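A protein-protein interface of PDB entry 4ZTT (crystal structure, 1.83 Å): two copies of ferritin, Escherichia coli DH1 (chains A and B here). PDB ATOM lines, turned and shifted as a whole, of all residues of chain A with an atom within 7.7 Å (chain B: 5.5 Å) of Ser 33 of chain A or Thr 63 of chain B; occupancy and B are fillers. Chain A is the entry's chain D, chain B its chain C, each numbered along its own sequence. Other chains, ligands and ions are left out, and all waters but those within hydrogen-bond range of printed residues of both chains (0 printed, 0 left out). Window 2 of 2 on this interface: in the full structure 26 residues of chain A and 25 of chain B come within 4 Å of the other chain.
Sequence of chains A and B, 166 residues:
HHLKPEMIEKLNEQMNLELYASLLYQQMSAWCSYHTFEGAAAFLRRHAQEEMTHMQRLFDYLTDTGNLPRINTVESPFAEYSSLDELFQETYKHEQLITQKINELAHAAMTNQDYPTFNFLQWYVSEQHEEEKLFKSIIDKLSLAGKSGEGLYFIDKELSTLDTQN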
ATOM      1  N   GLN A  26     -28.708  13.746  10.385  1.00  0.00           N
ATOM      2  CA  GLN A  26     -28.088  13.052  11.492  1.00  0.00           C
ATOM      3  C   GLN A  26     -29.161  12.299  12.362  1.00  0.00           C
ATOM      4  O   GLN A  26     -29.037  11.100  12.631  1.00  0.00           O
ATOM      5  CB  GLN A  26     -27.327  14.047  12.369  1.00  0.00           C
ATOM      6  CG  GLN A  26     -26.500  13.372  13.440  1.00  0.00           C
ATOM      7  CD  GLN A  26     -25.292  12.525  12.983  1.00  0.00           C
ATOM      8  OE1 GLN A  26     -25.010  11.438  13.563  1.00  0.00           O
ATOM      9  NE2 GLN A  26     -24.605  12.969  11.976  1.00  0.00           N
ATOM     10  N   GLN A  27     -30.216  12.998  12.696  1.00  0.00           N
ATOM     11  CA  GLN A  27     -31.302  12.522  13.550  1.00  0.00           C
ATOM     12  C   GLN A  27     -32.056  11.430  12.796  1.00  0.00           C
ATOM     13  O   GLN A  27     -32.374  10.343  13.350  1.00  0.00           O
ATOM     14  CB  GLN A  27     -32.251  13.636  13.907  1.00  0.00           C
ATOM     15  CG  GLN A  27     -33.351  13.169  14.824  1.00  0.00           C
ATOM     16  CD  GLN A  27     -32.741  12.797  16.179  1.00  0.00           C
ATOM     17  OE1 GLN A  27     -32.212  13.660  16.881  1.00  0.00           O
ATOM     18  NE2 GLN A  27     -32.840  11.545  16.560  1.00  0.00           N
ATOM     19  N   MET A  28     -32.286  11.642  11.507  1.00  0.00           N
ATOM     20  CA  MET A  28     -32.807  10.529  10.666  1.00  0.00           C
ATOM     21  C   MET A  28     -31.914   9.306  10.661  1.00  0.00           C
ATOM     22  O   MET A  28     -32.423   8.151  10.661  1.00  0.00           O
ATOM     23  CB  MET A  28     -33.122  10.988   9.243  1.00  0.00           C
ATOM     24  CG  MET A  28     -34.257  12.007   9.138  1.00  0.00           C
ATOM     25  SD  MET A  28     -34.199  12.646   7.473  1.00  0.00           S
ATOM     26  CE  MET A  28     -35.816  13.300   7.296  1.00  0.00           C
ATOM     27  N   SER A  29     -30.593   9.455  10.662  1.00  0.00           N
ATOM     28  CA  SER A  29     -29.716   8.260  10.649  1.00  0.00           C
ATOM     29  C   SER A  29     -29.987   7.448  11.943  1.00  0.00           C
ATOM     30  O   SER A  29     -29.834   6.221  11.934  1.00  0.00           O
ATOM     31  CB  SER A  29     -28.197   8.535  10.547  1.00  0.00           C
ATOM     32  OG  SER A  29     -27.629   8.947  11.813  1.00  0.00           O
ATOM     33  N   ALA A  30     -30.348   8.086  13.040  1.00  0.00           N
ATOM     34  CA  ALA A  30     -30.689   7.365  14.262  1.00  0.00           C
ATOM     35  C   ALA A  30     -31.920   6.559  14.124  1.00  0.00           C
ATOM     36  O   ALA A  30     -31.980   5.386  14.545  1.00  0.00           O
ATOM     37  CB  ALA A  30     -30.871   8.303  15.482  1.00  0.00           C
ATOM     38  N   TRP A  31     -32.971   7.148  13.558  1.00  0.00           N
ATOM     39  CA  TRP A  31     -34.159   6.349  13.270  1.00  0.00           C
ATOM     40  C   TRP A  31     -33.818   5.116  12.479  1.00  0.00           C
ATOM     41  O   TRP A  31     -34.326   4.009  12.771  1.00  0.00           O
ATOM     42  CB  TRP A  31     -35.220   7.174  12.525  1.00  0.00           C
ATOM     43  CG  TRP A  31     -36.576   6.505  12.358  1.00  0.00           C
ATOM     44  CD1 TRP A  31     -37.629   6.691  13.163  1.00  0.00           C
ATOM     45  CD2 TRP A  31     -36.976   5.582  11.361  1.00  0.00           C
ATOM     46  NE1 TRP A  31     -38.680   5.929  12.729  1.00  0.00           N
ATOM     47  CE2 TRP A  31     -38.310   5.250  11.617  1.00  0.00           C
ATOM     48  CE3 TRP A  31     -36.339   4.996  10.260  1.00  0.00           C
ATOM     49  CZ2 TRP A  31     -39.028   4.378  10.794  1.00  0.00           C
ATOM     50  CZ3 TRP A  31     -37.050   4.087   9.453  1.00  0.00           C
ATOM     51  CH2 TRP A  31     -38.386   3.804   9.718  1.00  0.00           C
ATOM     52  N   CYS A  32     -33.025   5.293  11.447  1.00  0.00           N
ATOM     53  CA  CYS A  32     -32.695   4.209  10.576  1.00  0.00           C
ATOM     54  C   CYS A  32     -31.933   3.107  11.337  1.00  0.00           C
ATOM     55  O   CYS A  32     -32.196   1.897  11.161  1.00  0.00           O
ATOM     56  CB  CYS A  32     -31.885   4.670   9.459  1.00  0.00           C
ATOM     57  SG  CYS A  32     -32.820   5.600   8.163  1.00  0.00           S
ATOM     58  N   SER A  33     -30.940   3.499  12.173  1.00  0.00           N
ATOM     59  CA  SER A  33     -30.193   2.521  12.985  1.00  0.00           C
ATOM     60  C   SER A  33     -31.122   1.750  13.898  1.00  0.00           C
ATOM     61  O   SER A  33     -31.028   0.501  13.937  1.00  0.00           O
ATOM     62  CB  SER A  33     -29.130   3.168  13.893  1.00  0.00           C
ATOM     63  OG  SER A  33     -28.121   3.640  13.090  1.00  0.00           O
ATOM     64  N   TYR A  34     -31.948   2.478  14.629  1.00  0.00           N
ATOM     65  CA  TYR A  34     -32.959   1.875  15.563  1.00  0.00           C
ATOM     66  C   TYR A  34     -33.874   0.887  14.880  1.00  0.00           C
ATOM     67  O   TYR A  34     -34.275  -0.141  15.499  1.00  0.00           O
ATOM     68  CB  TYR A  34     -33.757   2.969  16.153  1.00  0.00           C
ATOM     69  CG  TYR A  34     -34.640   2.596  17.314  1.00  0.00           C
ATOM     70  CD1 TYR A  34     -34.110   2.314  18.549  1.00  0.00           C
ATOM     71  CD2 TYR A  34     -36.014   2.522  17.157  1.00  0.00           C
ATOM     72  CE1 TYR A  34     -34.955   1.998  19.651  1.00  0.00           C
ATOM     73  CE2 TYR A  34     -36.853   2.193  18.220  1.00  0.00           C
ATOM     74  CZ  TYR A  34     -36.310   1.918  19.477  1.00  0.00           C
ATOM     75  OH  TYR A  34     -37.113   1.610  20.553  1.00  0.00           O
ATOM     76  N   HIS A  35     -34.240   1.164  13.631  1.00  0.00           N
ATOM     77  CA  HIS A  35     -35.076   0.251  12.836  1.00  0.00           C
ATOM     78  C   HIS A  35     -34.328  -0.732  11.988  1.00  0.00           C
ATOM     79  O   HIS A  35     -34.908  -1.376  11.167  1.00  0.00           O
ATOM     80  CB  HIS A  35     -36.067   1.071  11.973  1.00  0.00           C
ATOM     81  CG  HIS A  35     -37.137   1.668  12.785  1.00  0.00           C
ATOM     82  ND1 HIS A  35     -37.017   2.906  13.403  1.00  0.00           N
ATOM     83  CD2 HIS A  35     -38.269   1.118  13.255  1.00  0.00           C
ATOM     84  CE1 HIS A  35     -38.078   3.118  14.156  1.00  0.00           C
ATOM     85  NE2 HIS A  35     -38.854   2.058  14.054  1.00  0.00           N
ATOM     86  N   THR A  36     -33.025  -0.821  12.209  1.00  0.00           N
ATOM     87  CA  THR A  36     -32.110  -1.826  11.628  1.00  0.00           C
ATOM     88  C   THR A  36     -31.657  -1.572  10.179  1.00  0.00           C
ATOM     89  O   THR A  36     -31.055  -2.428   9.566  1.00  0.00           O
ATOM     90  CB  THR A  36     -32.604  -3.283  11.784  1.00  0.00           C
ATOM     91  OG1 THR A  36     -33.476  -3.623  10.725  1.00  0.00           O
ATOM     92  CG2 THR A  36     -33.293  -3.516  13.148  1.00  0.00           C
ATOM     93  N   PHE A  37     -31.901  -0.366   9.652  1.00  0.00           N
ATOM     94  CA  PHE A  37     -31.406  -0.025   8.310  1.00  0.00           C
ATOM     95  C   PHE A  37     -30.106   0.640   8.469  1.00  0.00           C
ATOM     96  O   PHE A  37     -30.014   1.882   8.411  1.00  0.00           O
ATOM     97  CB  PHE A  37     -32.442   0.881   7.623  1.00  0.00           C
ATOM     98  CG  PHE A  37     -33.767   0.279   7.521  1.00  0.00           C
ATOM     99  CD1 PHE A  37     -33.957  -0.829   6.698  1.00  0.00           C
ATOM    100  CD2 PHE A  37     -34.835   0.791   8.194  1.00  0.00           C
ATOM    101  CE1 PHE A  37     -35.218  -1.410   6.565  1.00  0.00           C
ATOM    102  CE2 PHE A  37     -36.113   0.230   8.090  1.00  0.00           C
ATOM    103  CZ  PHE A  37     -36.277  -0.927   7.336  1.00  0.00           C
ATOM    104  N   GLU A  38     -29.047  -0.156   8.620  1.00  0.00           N
ATOM    105  CA  GLU A  38     -27.793   0.408   8.951  1.00  0.00           C
ATOM    106  C   GLU A  38     -27.143   1.023   7.705  1.00  0.00           C
ATOM    107  O   GLU A  38     -26.288   1.861   7.848  1.00  0.00           O
ATOM    108  CB  GLU A  38     -26.878  -0.676   9.579  1.00  0.00           C
ATOM    109  CG  GLU A  38     -27.270  -1.071  11.008  1.00  0.00           C
ATOM    110  CD  GLU A  38     -27.135   0.069  12.041  1.00  0.00           C
ATOM    111  OE1 GLU A  38     -26.383   1.077  11.864  1.00  0.00           O
ATOM    112  OE2 GLU A  38     -27.835   0.008  13.063  1.00  0.00           O
ATOM    113  N   GLY A  39     -27.429   0.512   6.502  1.00  0.00           N
ATOM    114  CA  GLY A  39     -26.975   1.100   5.275  1.00  0.00           C
ATOM    115  C   GLY A  39     -27.570   2.515   5.053  1.00  0.00           C
ATOM    116  O   GLY A  39     -26.805   3.442   4.741  1.00  0.00           O
ATOM    117  N   ALA A  40     -28.899   2.674   5.195  1.00  0.00           N
ATOM    118  CA  ALA A  40     -29.592   3.955   5.164  1.00  0.00           C
ATOM    119  C   ALA A  40     -28.979   4.893   6.240  1.00  0.00           C
ATOM    120  O   ALA A  40     -28.689   6.054   5.926  1.00  0.00           O
ATOM    121  CB  ALA A  40     -31.024   3.759   5.477  1.00  0.00           C
ATOM    122  N   ALA A  41     -28.627   4.332   7.403  1.00  0.00           N
ATOM    123  CA  ALA A  41     -28.076   5.158   8.509  1.00  0.00           C
ATOM    124  C   ALA A  41     -26.729   5.688   8.066  1.00  0.00           C
ATOM    125  O   ALA A  41     -26.442   6.902   8.267  1.00  0.00           O
ATOM    126  CB  ALA A  41     -27.985   4.371   9.826  1.00  0.00           C
ATOM    127  N   ALA A  42     -25.924   4.882   7.441  1.00  0.00           N
ATOM    128  CA  ALA A  42     -24.586   5.273   7.021  1.00  0.00           C
ATOM    129  C   ALA A  42     -24.644   6.364   5.917  1.00  0.00           C
ATOM    130  O   ALA A  42     -23.858   7.323   5.903  1.00  0.00           O
ATOM    131  CB  ALA A  42     -23.840   4.113   6.536  1.00  0.00           C
ATOM    132  N   LEU A  44     -27.092   8.547   5.417  1.00  0.00           N
ATOM    133  CA  LEU A  44     -27.558   9.778   6.096  1.00  0.00           C
ATOM    134  C   LEU A  44     -26.453  10.393   6.978  1.00  0.00           C
ATOM    135  O   LEU A  44     -26.303  11.659   7.039  1.00  0.00           O
ATOM    136  CB  LEU A  44     -28.822   9.514   6.890  1.00  0.00           C
ATOM    137  CG  LEU A  44     -30.076   9.234   6.059  1.00  0.00           C
ATOM    138  CD1 LEU A  44     -31.101   8.543   6.874  1.00  0.00           C
ATOM    139  CD2 LEU A  44     -30.642  10.438   5.366  1.00  0.00           C
ATOM    140  N   ARG A  45     -25.706   9.564   7.734  1.00  0.00           N
ATOM    141  CA  ARG A  45     -24.519  10.129   8.462  1.00  0.00           C
ATOM    142  C   ARG A  45     -23.542  10.816   7.558  1.00  0.00           C
ATOM    143  O   ARG A  45     -23.125  11.927   7.818  1.00  0.00           O
ATOM    144  CB  ARG A  45     -23.839   8.971   9.270  1.00  0.00           C
ATOM    145  CG  ARG A  45     -22.895   9.138  10.434  1.00  0.00           C
ATOM    146  CD  ARG A  45     -23.219   7.872  11.350  1.00  0.00           C
ATOM    147  NE  ARG A  45     -22.905   6.626  10.650  1.00  0.00           N
ATOM    148  CZ  ARG A  45     -23.544   5.457  10.704  1.00  0.00           C
ATOM    149  NH1 ARG A  45     -23.037   4.479  10.032  1.00  0.00           N
ATOM    150  NH2 ARG A  45     -24.678   5.235  11.342  1.00  0.00           N
ATOM    151  N   LEU A  87     -39.544   8.384   5.527  1.00  0.00           N
ATOM    152  CA  LEU A  87     -38.328   9.162   5.924  1.00  0.00           C
ATOM    153  C   LEU A  87     -37.661   9.739   4.662  1.00  0.00           C
ATOM    154  O   LEU A  87     -37.267  10.958   4.654  1.00  0.00           O
ATOM    155  CB  LEU A  87     -37.380   8.260   6.749  1.00  0.00           C
ATOM    156  CG  LEU A  87     -36.129   8.948   7.300  1.00  0.00           C
ATOM    157  CD1 LEU A  87     -35.699   8.110   8.513  1.00  0.00           C
ATOM    158  CD2 LEU A  87     -35.080   8.917   6.248  1.00  0.00           C
ATOM    159  N   ASP A 156     -31.164  -1.135   1.332  1.00  0.00           N
ATOM    160  CA  ASP A 156     -30.321  -0.781   2.476  1.00  0.00           C
ATOM    161  C   ASP A 156     -28.849  -1.030   2.162  1.00  0.00           C
ATOM    162  O   ASP A 156     -27.982  -0.220   2.447  1.00  0.00           O
ATOM    163  CB  ASP A 156     -30.771  -1.468   3.713  1.00  0.00           C
ATOM    164  CG  ASP A 156     -30.027  -0.998   4.913  1.00  0.00           C
ATOM    165  OD1 ASP A 156     -30.319   0.126   5.368  1.00  0.00           O
ATOM    166  OD2 ASP A 156     -29.122  -1.702   5.351  1.00  0.00           O
ATOM    167  N   LEU B  58     -20.586   9.318  20.732  1.00  0.00           N
ATOM    168  CA  LEU B  58     -21.644   9.089  21.657  1.00  0.00           C
ATOM    169  C   LEU B  58     -22.939   8.636  20.968  1.00  0.00           C
ATOM    170  O   LEU B  58     -23.660   7.712  21.402  1.00  0.00           O
ATOM    171  CB  LEU B  58     -21.893  10.405  22.390  1.00  0.00           C
ATOM    172  CG  LEU B  58     -20.944  10.562  23.612  1.00  0.00           C
ATOM    173  CD1 LEU B  58     -20.655  12.048  23.865  1.00  0.00           C
ATOM    174  CD2 LEU B  58     -21.485   9.939  24.930  1.00  0.00           C
ATOM    175  N   PHE B  59     -23.254   9.316  19.862  1.00  0.00           N
ATOM    176  CA  PHE B  59     -24.414   8.908  18.980  1.00  0.00           C
ATOM    177  C   PHE B  59     -24.366   7.393  18.649  1.00  0.00           C
ATOM    178  O   PHE B  59     -25.359   6.675  18.829  1.00  0.00           O
ATOM    179  CB  PHE B  59     -24.402   9.866  17.751  1.00  0.00           C
ATOM    180  CG  PHE B  59     -25.692   9.931  16.975  1.00  0.00           C
ATOM    181  CD1 PHE B  59     -25.988   8.974  16.057  1.00  0.00           C
ATOM    182  CD2 PHE B  59     -26.507  11.008  17.137  1.00  0.00           C
ATOM    183  CE1 PHE B  59     -27.151   9.116  15.243  1.00  0.00           C
ATOM    184  CE2 PHE B  59     -27.680  11.148  16.431  1.00  0.00           C
ATOM    185  CZ  PHE B  59     -27.977  10.192  15.487  1.00  0.00           C
ATOM    186  N   ASP B  60     -23.227   6.927  18.213  1.00  0.00           N
ATOM    187  CA  ASP B  60     -22.974   5.574  17.844  1.00  0.00           C
ATOM    188  C   ASP B  60     -23.116   4.611  19.021  1.00  0.00           C
ATOM    189  O   ASP B  60     -23.578   3.436  18.867  1.00  0.00           O
ATOM    190  CB  ASP B  60     -21.599   5.415  17.186  1.00  0.00           C
ATOM    191  CG  ASP B  60     -21.512   6.061  15.780  1.00  0.00           C
ATOM    192  OD1 ASP B  60     -22.492   6.479  15.240  1.00  0.00           O
ATOM    193  OD2 ASP B  60     -20.413   6.216  15.329  1.00  0.00           O
ATOM    194  N   TYR B  61     -22.653   5.036  20.212  1.00  0.00           N
ATOM    195  CA  TYR B  61     -22.735   4.137  21.379  1.00  0.00           C
ATOM    196  C   TYR B  61     -24.214   3.981  21.738  1.00  0.00           C
ATOM    197  O   TYR B  61     -24.689   2.864  22.074  1.00  0.00           O
ATOM    198  CB  TYR B  61     -21.921   4.721  22.619  1.00  0.00           C
ATOM    199  CG  TYR B  61     -21.974   3.857  23.831  1.00  0.00           C
ATOM    200  CD1 TYR B  61     -21.271   2.663  23.885  1.00  0.00           C
ATOM    201  CD2 TYR B  61     -22.677   4.238  24.991  1.00  0.00           C
ATOM    202  CE1 TYR B  61     -21.344   1.839  24.930  1.00  0.00           C
ATOM    203  CE2 TYR B  61     -22.746   3.410  26.104  1.00  0.00           C
ATOM    204  CZ  TYR B  61     -22.011   2.212  26.073  1.00  0.00           C
ATOM    205  OH  TYR B  61     -22.002   1.389  27.098  1.00  0.00           O
ATOM    206  N   LEU B  62     -24.940   5.068  21.635  1.00  0.00           N
ATOM    207  CA  LEU B  62     -26.361   5.065  21.937  1.00  0.00           C
ATOM    208  C   LEU B  62     -27.127   4.153  20.954  1.00  0.00           C
ATOM    209  O   LEU B  62     -27.942   3.299  21.440  1.00  0.00           O
ATOM    210  CB  LEU B  62     -26.911   6.466  22.006  1.00  0.00           C
ATOM    211  CG  LEU B  62     -26.651   7.130  23.407  1.00  0.00           C
ATOM    212  CD1 LEU B  62     -26.858   8.595  23.230  1.00  0.00           C
ATOM    213  CD2 LEU B  62     -27.552   6.624  24.490  1.00  0.00           C
ATOM    214  N   THR B  63     -26.840   4.261  19.621  1.00  0.00           N
ATOM    215  CA  THR B  63     -27.533   3.452  18.656  1.00  0.00           C
ATOM    216  C   THR B  63     -27.098   1.972  18.789  1.00  0.00           C
ATOM    217  O   THR B  63     -27.973   1.113  18.790  1.00  0.00           O
ATOM    218  CB  THR B  63     -27.377   3.927  17.183  1.00  0.00           C
ATOM    219  OG1 THR B  63     -26.040   3.895  16.846  1.00  0.00           O
ATOM    220  CG2 THR B  63     -27.828   5.239  17.013  1.00  0.00           C
ATOM    221  N   ASP B  64     -25.794   1.706  19.026  1.00  0.00           N
ATOM    222  CA  ASP B  64     -25.268   0.389  19.280  1.00  0.00           C
ATOM    223  C   ASP B  64     -25.916  -0.325  20.403  1.00  0.00           C
ATOM    224  O   ASP B  64     -26.140  -1.534  20.324  1.00  0.00           O
ATOM    225  CB  ASP B  64     -23.760   0.342  19.507  1.00  0.00           C
ATOM    226  CG  ASP B  64     -22.930   0.662  18.302  1.00  0.00           C
ATOM    227  OD1 ASP B  64     -23.423   0.709  17.195  1.00  0.00           O
ATOM    228  OD2 ASP B  64     -21.707   0.856  18.500  1.00  0.00           O
ATOM    229  N   THR B  65     -26.262   0.355  21.439  1.00  0.00           N
ATOM    230  CA  THR B  65     -26.897  -0.245  22.598  1.00  0.00           C
ATOM    231  C   THR B  65     -28.429  -0.325  22.537  1.00  0.00           C
ATOM    232  O   THR B  65     -29.039  -0.696  23.492  1.00  0.00           O
ATOM    233  CB  THR B  65     -26.472   0.456  23.874  1.00  0.00           C
ATOM    234  OG1 THR B  65     -26.854   1.827  23.866  1.00  0.00           O
ATOM    235  CG2 THR B  65     -24.912   0.433  24.111  1.00  0.00           C
ATOM    236  N   GLY B  66     -29.018   0.042  21.405  1.00  0.00           N
ATOM    237  CA  GLY B  66     -30.449  -0.151  21.157  1.00  0.00           C
ATOM    238  C   GLY B  66     -31.237   1.063  21.537  1.00  0.00           C
ATOM    239  O   GLY B  66     -32.465   0.992  21.712  1.00  0.00           O
ATOM    240  N   ASN B  67     -30.578   2.222  21.627  1.00  0.00           N
ATOM    241  CA  ASN B  67     -31.281   3.442  22.069  1.00  0.00           C
ATOM    242  C   ASN B  67     -31.391   4.417  20.872  1.00  0.00           C
ATOM    243  O   ASN B  67     -30.780   4.220  19.832  1.00  0.00           O
ATOM    244  CB  ASN B  67     -30.594   4.043  23.319  1.00  0.00           C
ATOM    245  CG  ASN B  67     -30.576   3.063  24.504  1.00  0.00           C
ATOM    246  OD1 ASN B  67     -29.534   2.461  24.825  1.00  0.00           O
ATOM    247  ND2 ASN B  67     -31.722   2.827  25.065  1.00  0.00           N
ATOM    248  N   PRO B  69     -30.622   8.028  20.042  1.00  0.00           N
ATOM    249  CA  PRO B  69     -30.199   9.382  20.452  1.00  0.00           C
ATOM    250  C   PRO B  69     -31.117  10.458  19.919  1.00  0.00           C
ATOM    251  O   PRO B  69     -31.779  10.253  18.842  1.00  0.00           O
ATOM    252  CB  PRO B  69     -28.794   9.516  19.898  1.00  0.00           C
ATOM    253  CG  PRO B  69     -28.696   8.490  18.832  1.00  0.00           C
ATOM    254  CD  PRO B  69     -29.734   7.437  19.083  1.00  0.00           C
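The side-chain carboxylate of Glu 38 of chain A lies within hydrogen-bond range of the side-chain hydroxyl of Ser 33 of chain A (3.3 Å).
The backbone carbonyl oxygen (O) of Gln 26 of chain A lies within hydrogen-bond range of the side-chain hydroxyl (OG) of Ser 29 of chain A.
The side-chain hydroxyl of Thr 63 of chain B lies within hydrogen-bond range of the backbone carbonyl oxygen of Asp 60 of chain B (3.2 Å).
The backbone carbonyl oxygen (O) of Ser 29 of chain A lies within hydrogen-bond range of the side-chain hydroxyl (OG) of Ser 33 of chain A (3.3 Å).
OG1 of Thr 63 of chain B sits close to O of Phe 59 of chain B (3.5 Å).
Of chain B, only Thr 63 (3.8 Å) comes within 4 Å of Ser 33 of chain A.
Of chain A, only Ser 33 (3.8 Å) comes within 4 Å of Thr 63 of chain B.
Printed residues of chain B within 4 Å of Gln 27 of chain A: Pro 69.
Printed residues of chain B within 4 Å of Tyr 34 of chain A: Gly 66.
Of the printed residues of chain A, Gly 66 of chain B touches Tyr 34.
The nearest printed residue of chain B that does not touch Ser 33 of chain A is Phe 59 of chain B (6.0 Å).
The nearest printed residue of chain B that does not touch Gln 27 of chain A is Phe 59 of chain B (4.5 Å).
No position is printed for both chains.
Of the 7 pairs that touch across the chains among the printed residues, none has its exchanged pair printed and touching as well.
Hydrophobic or aromatic side chains of chain A within 4 Å of the printed part of chain B: Ala 30 and Tyr 34.
Of the 11 printed residues of chain B, 4 touch a printed residue of chain A.
Among the printed residues, 7 pairs touch across the chains.
Among the printed residues, no Asp or Glu carboxylate lies within 4 Å of a Lys or Arg side-chain nitrogen of the other chain.
Among the printed residues, merely in contact across the chains: Gln 26 of chain A with Phe 59 of chain B (3.2 Å), Tyr 34 of chain A with Gly 66 of chain B (3.4 Å), Ala 30 of chain A with Phe 59 of chain B (3.5 Å), Ser 29 of chain A with Phe 59 of chain B (3.5 Å), Ser 33 of chain A with Thr 63 of chain B (3.8 Å) and Ala 30 of chain A with Pro 69 of chain B (3.9 Å).
O of Pro 69 of chain B lies within hydrogen-bond range of NE2 of Gln 27 of chain A.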
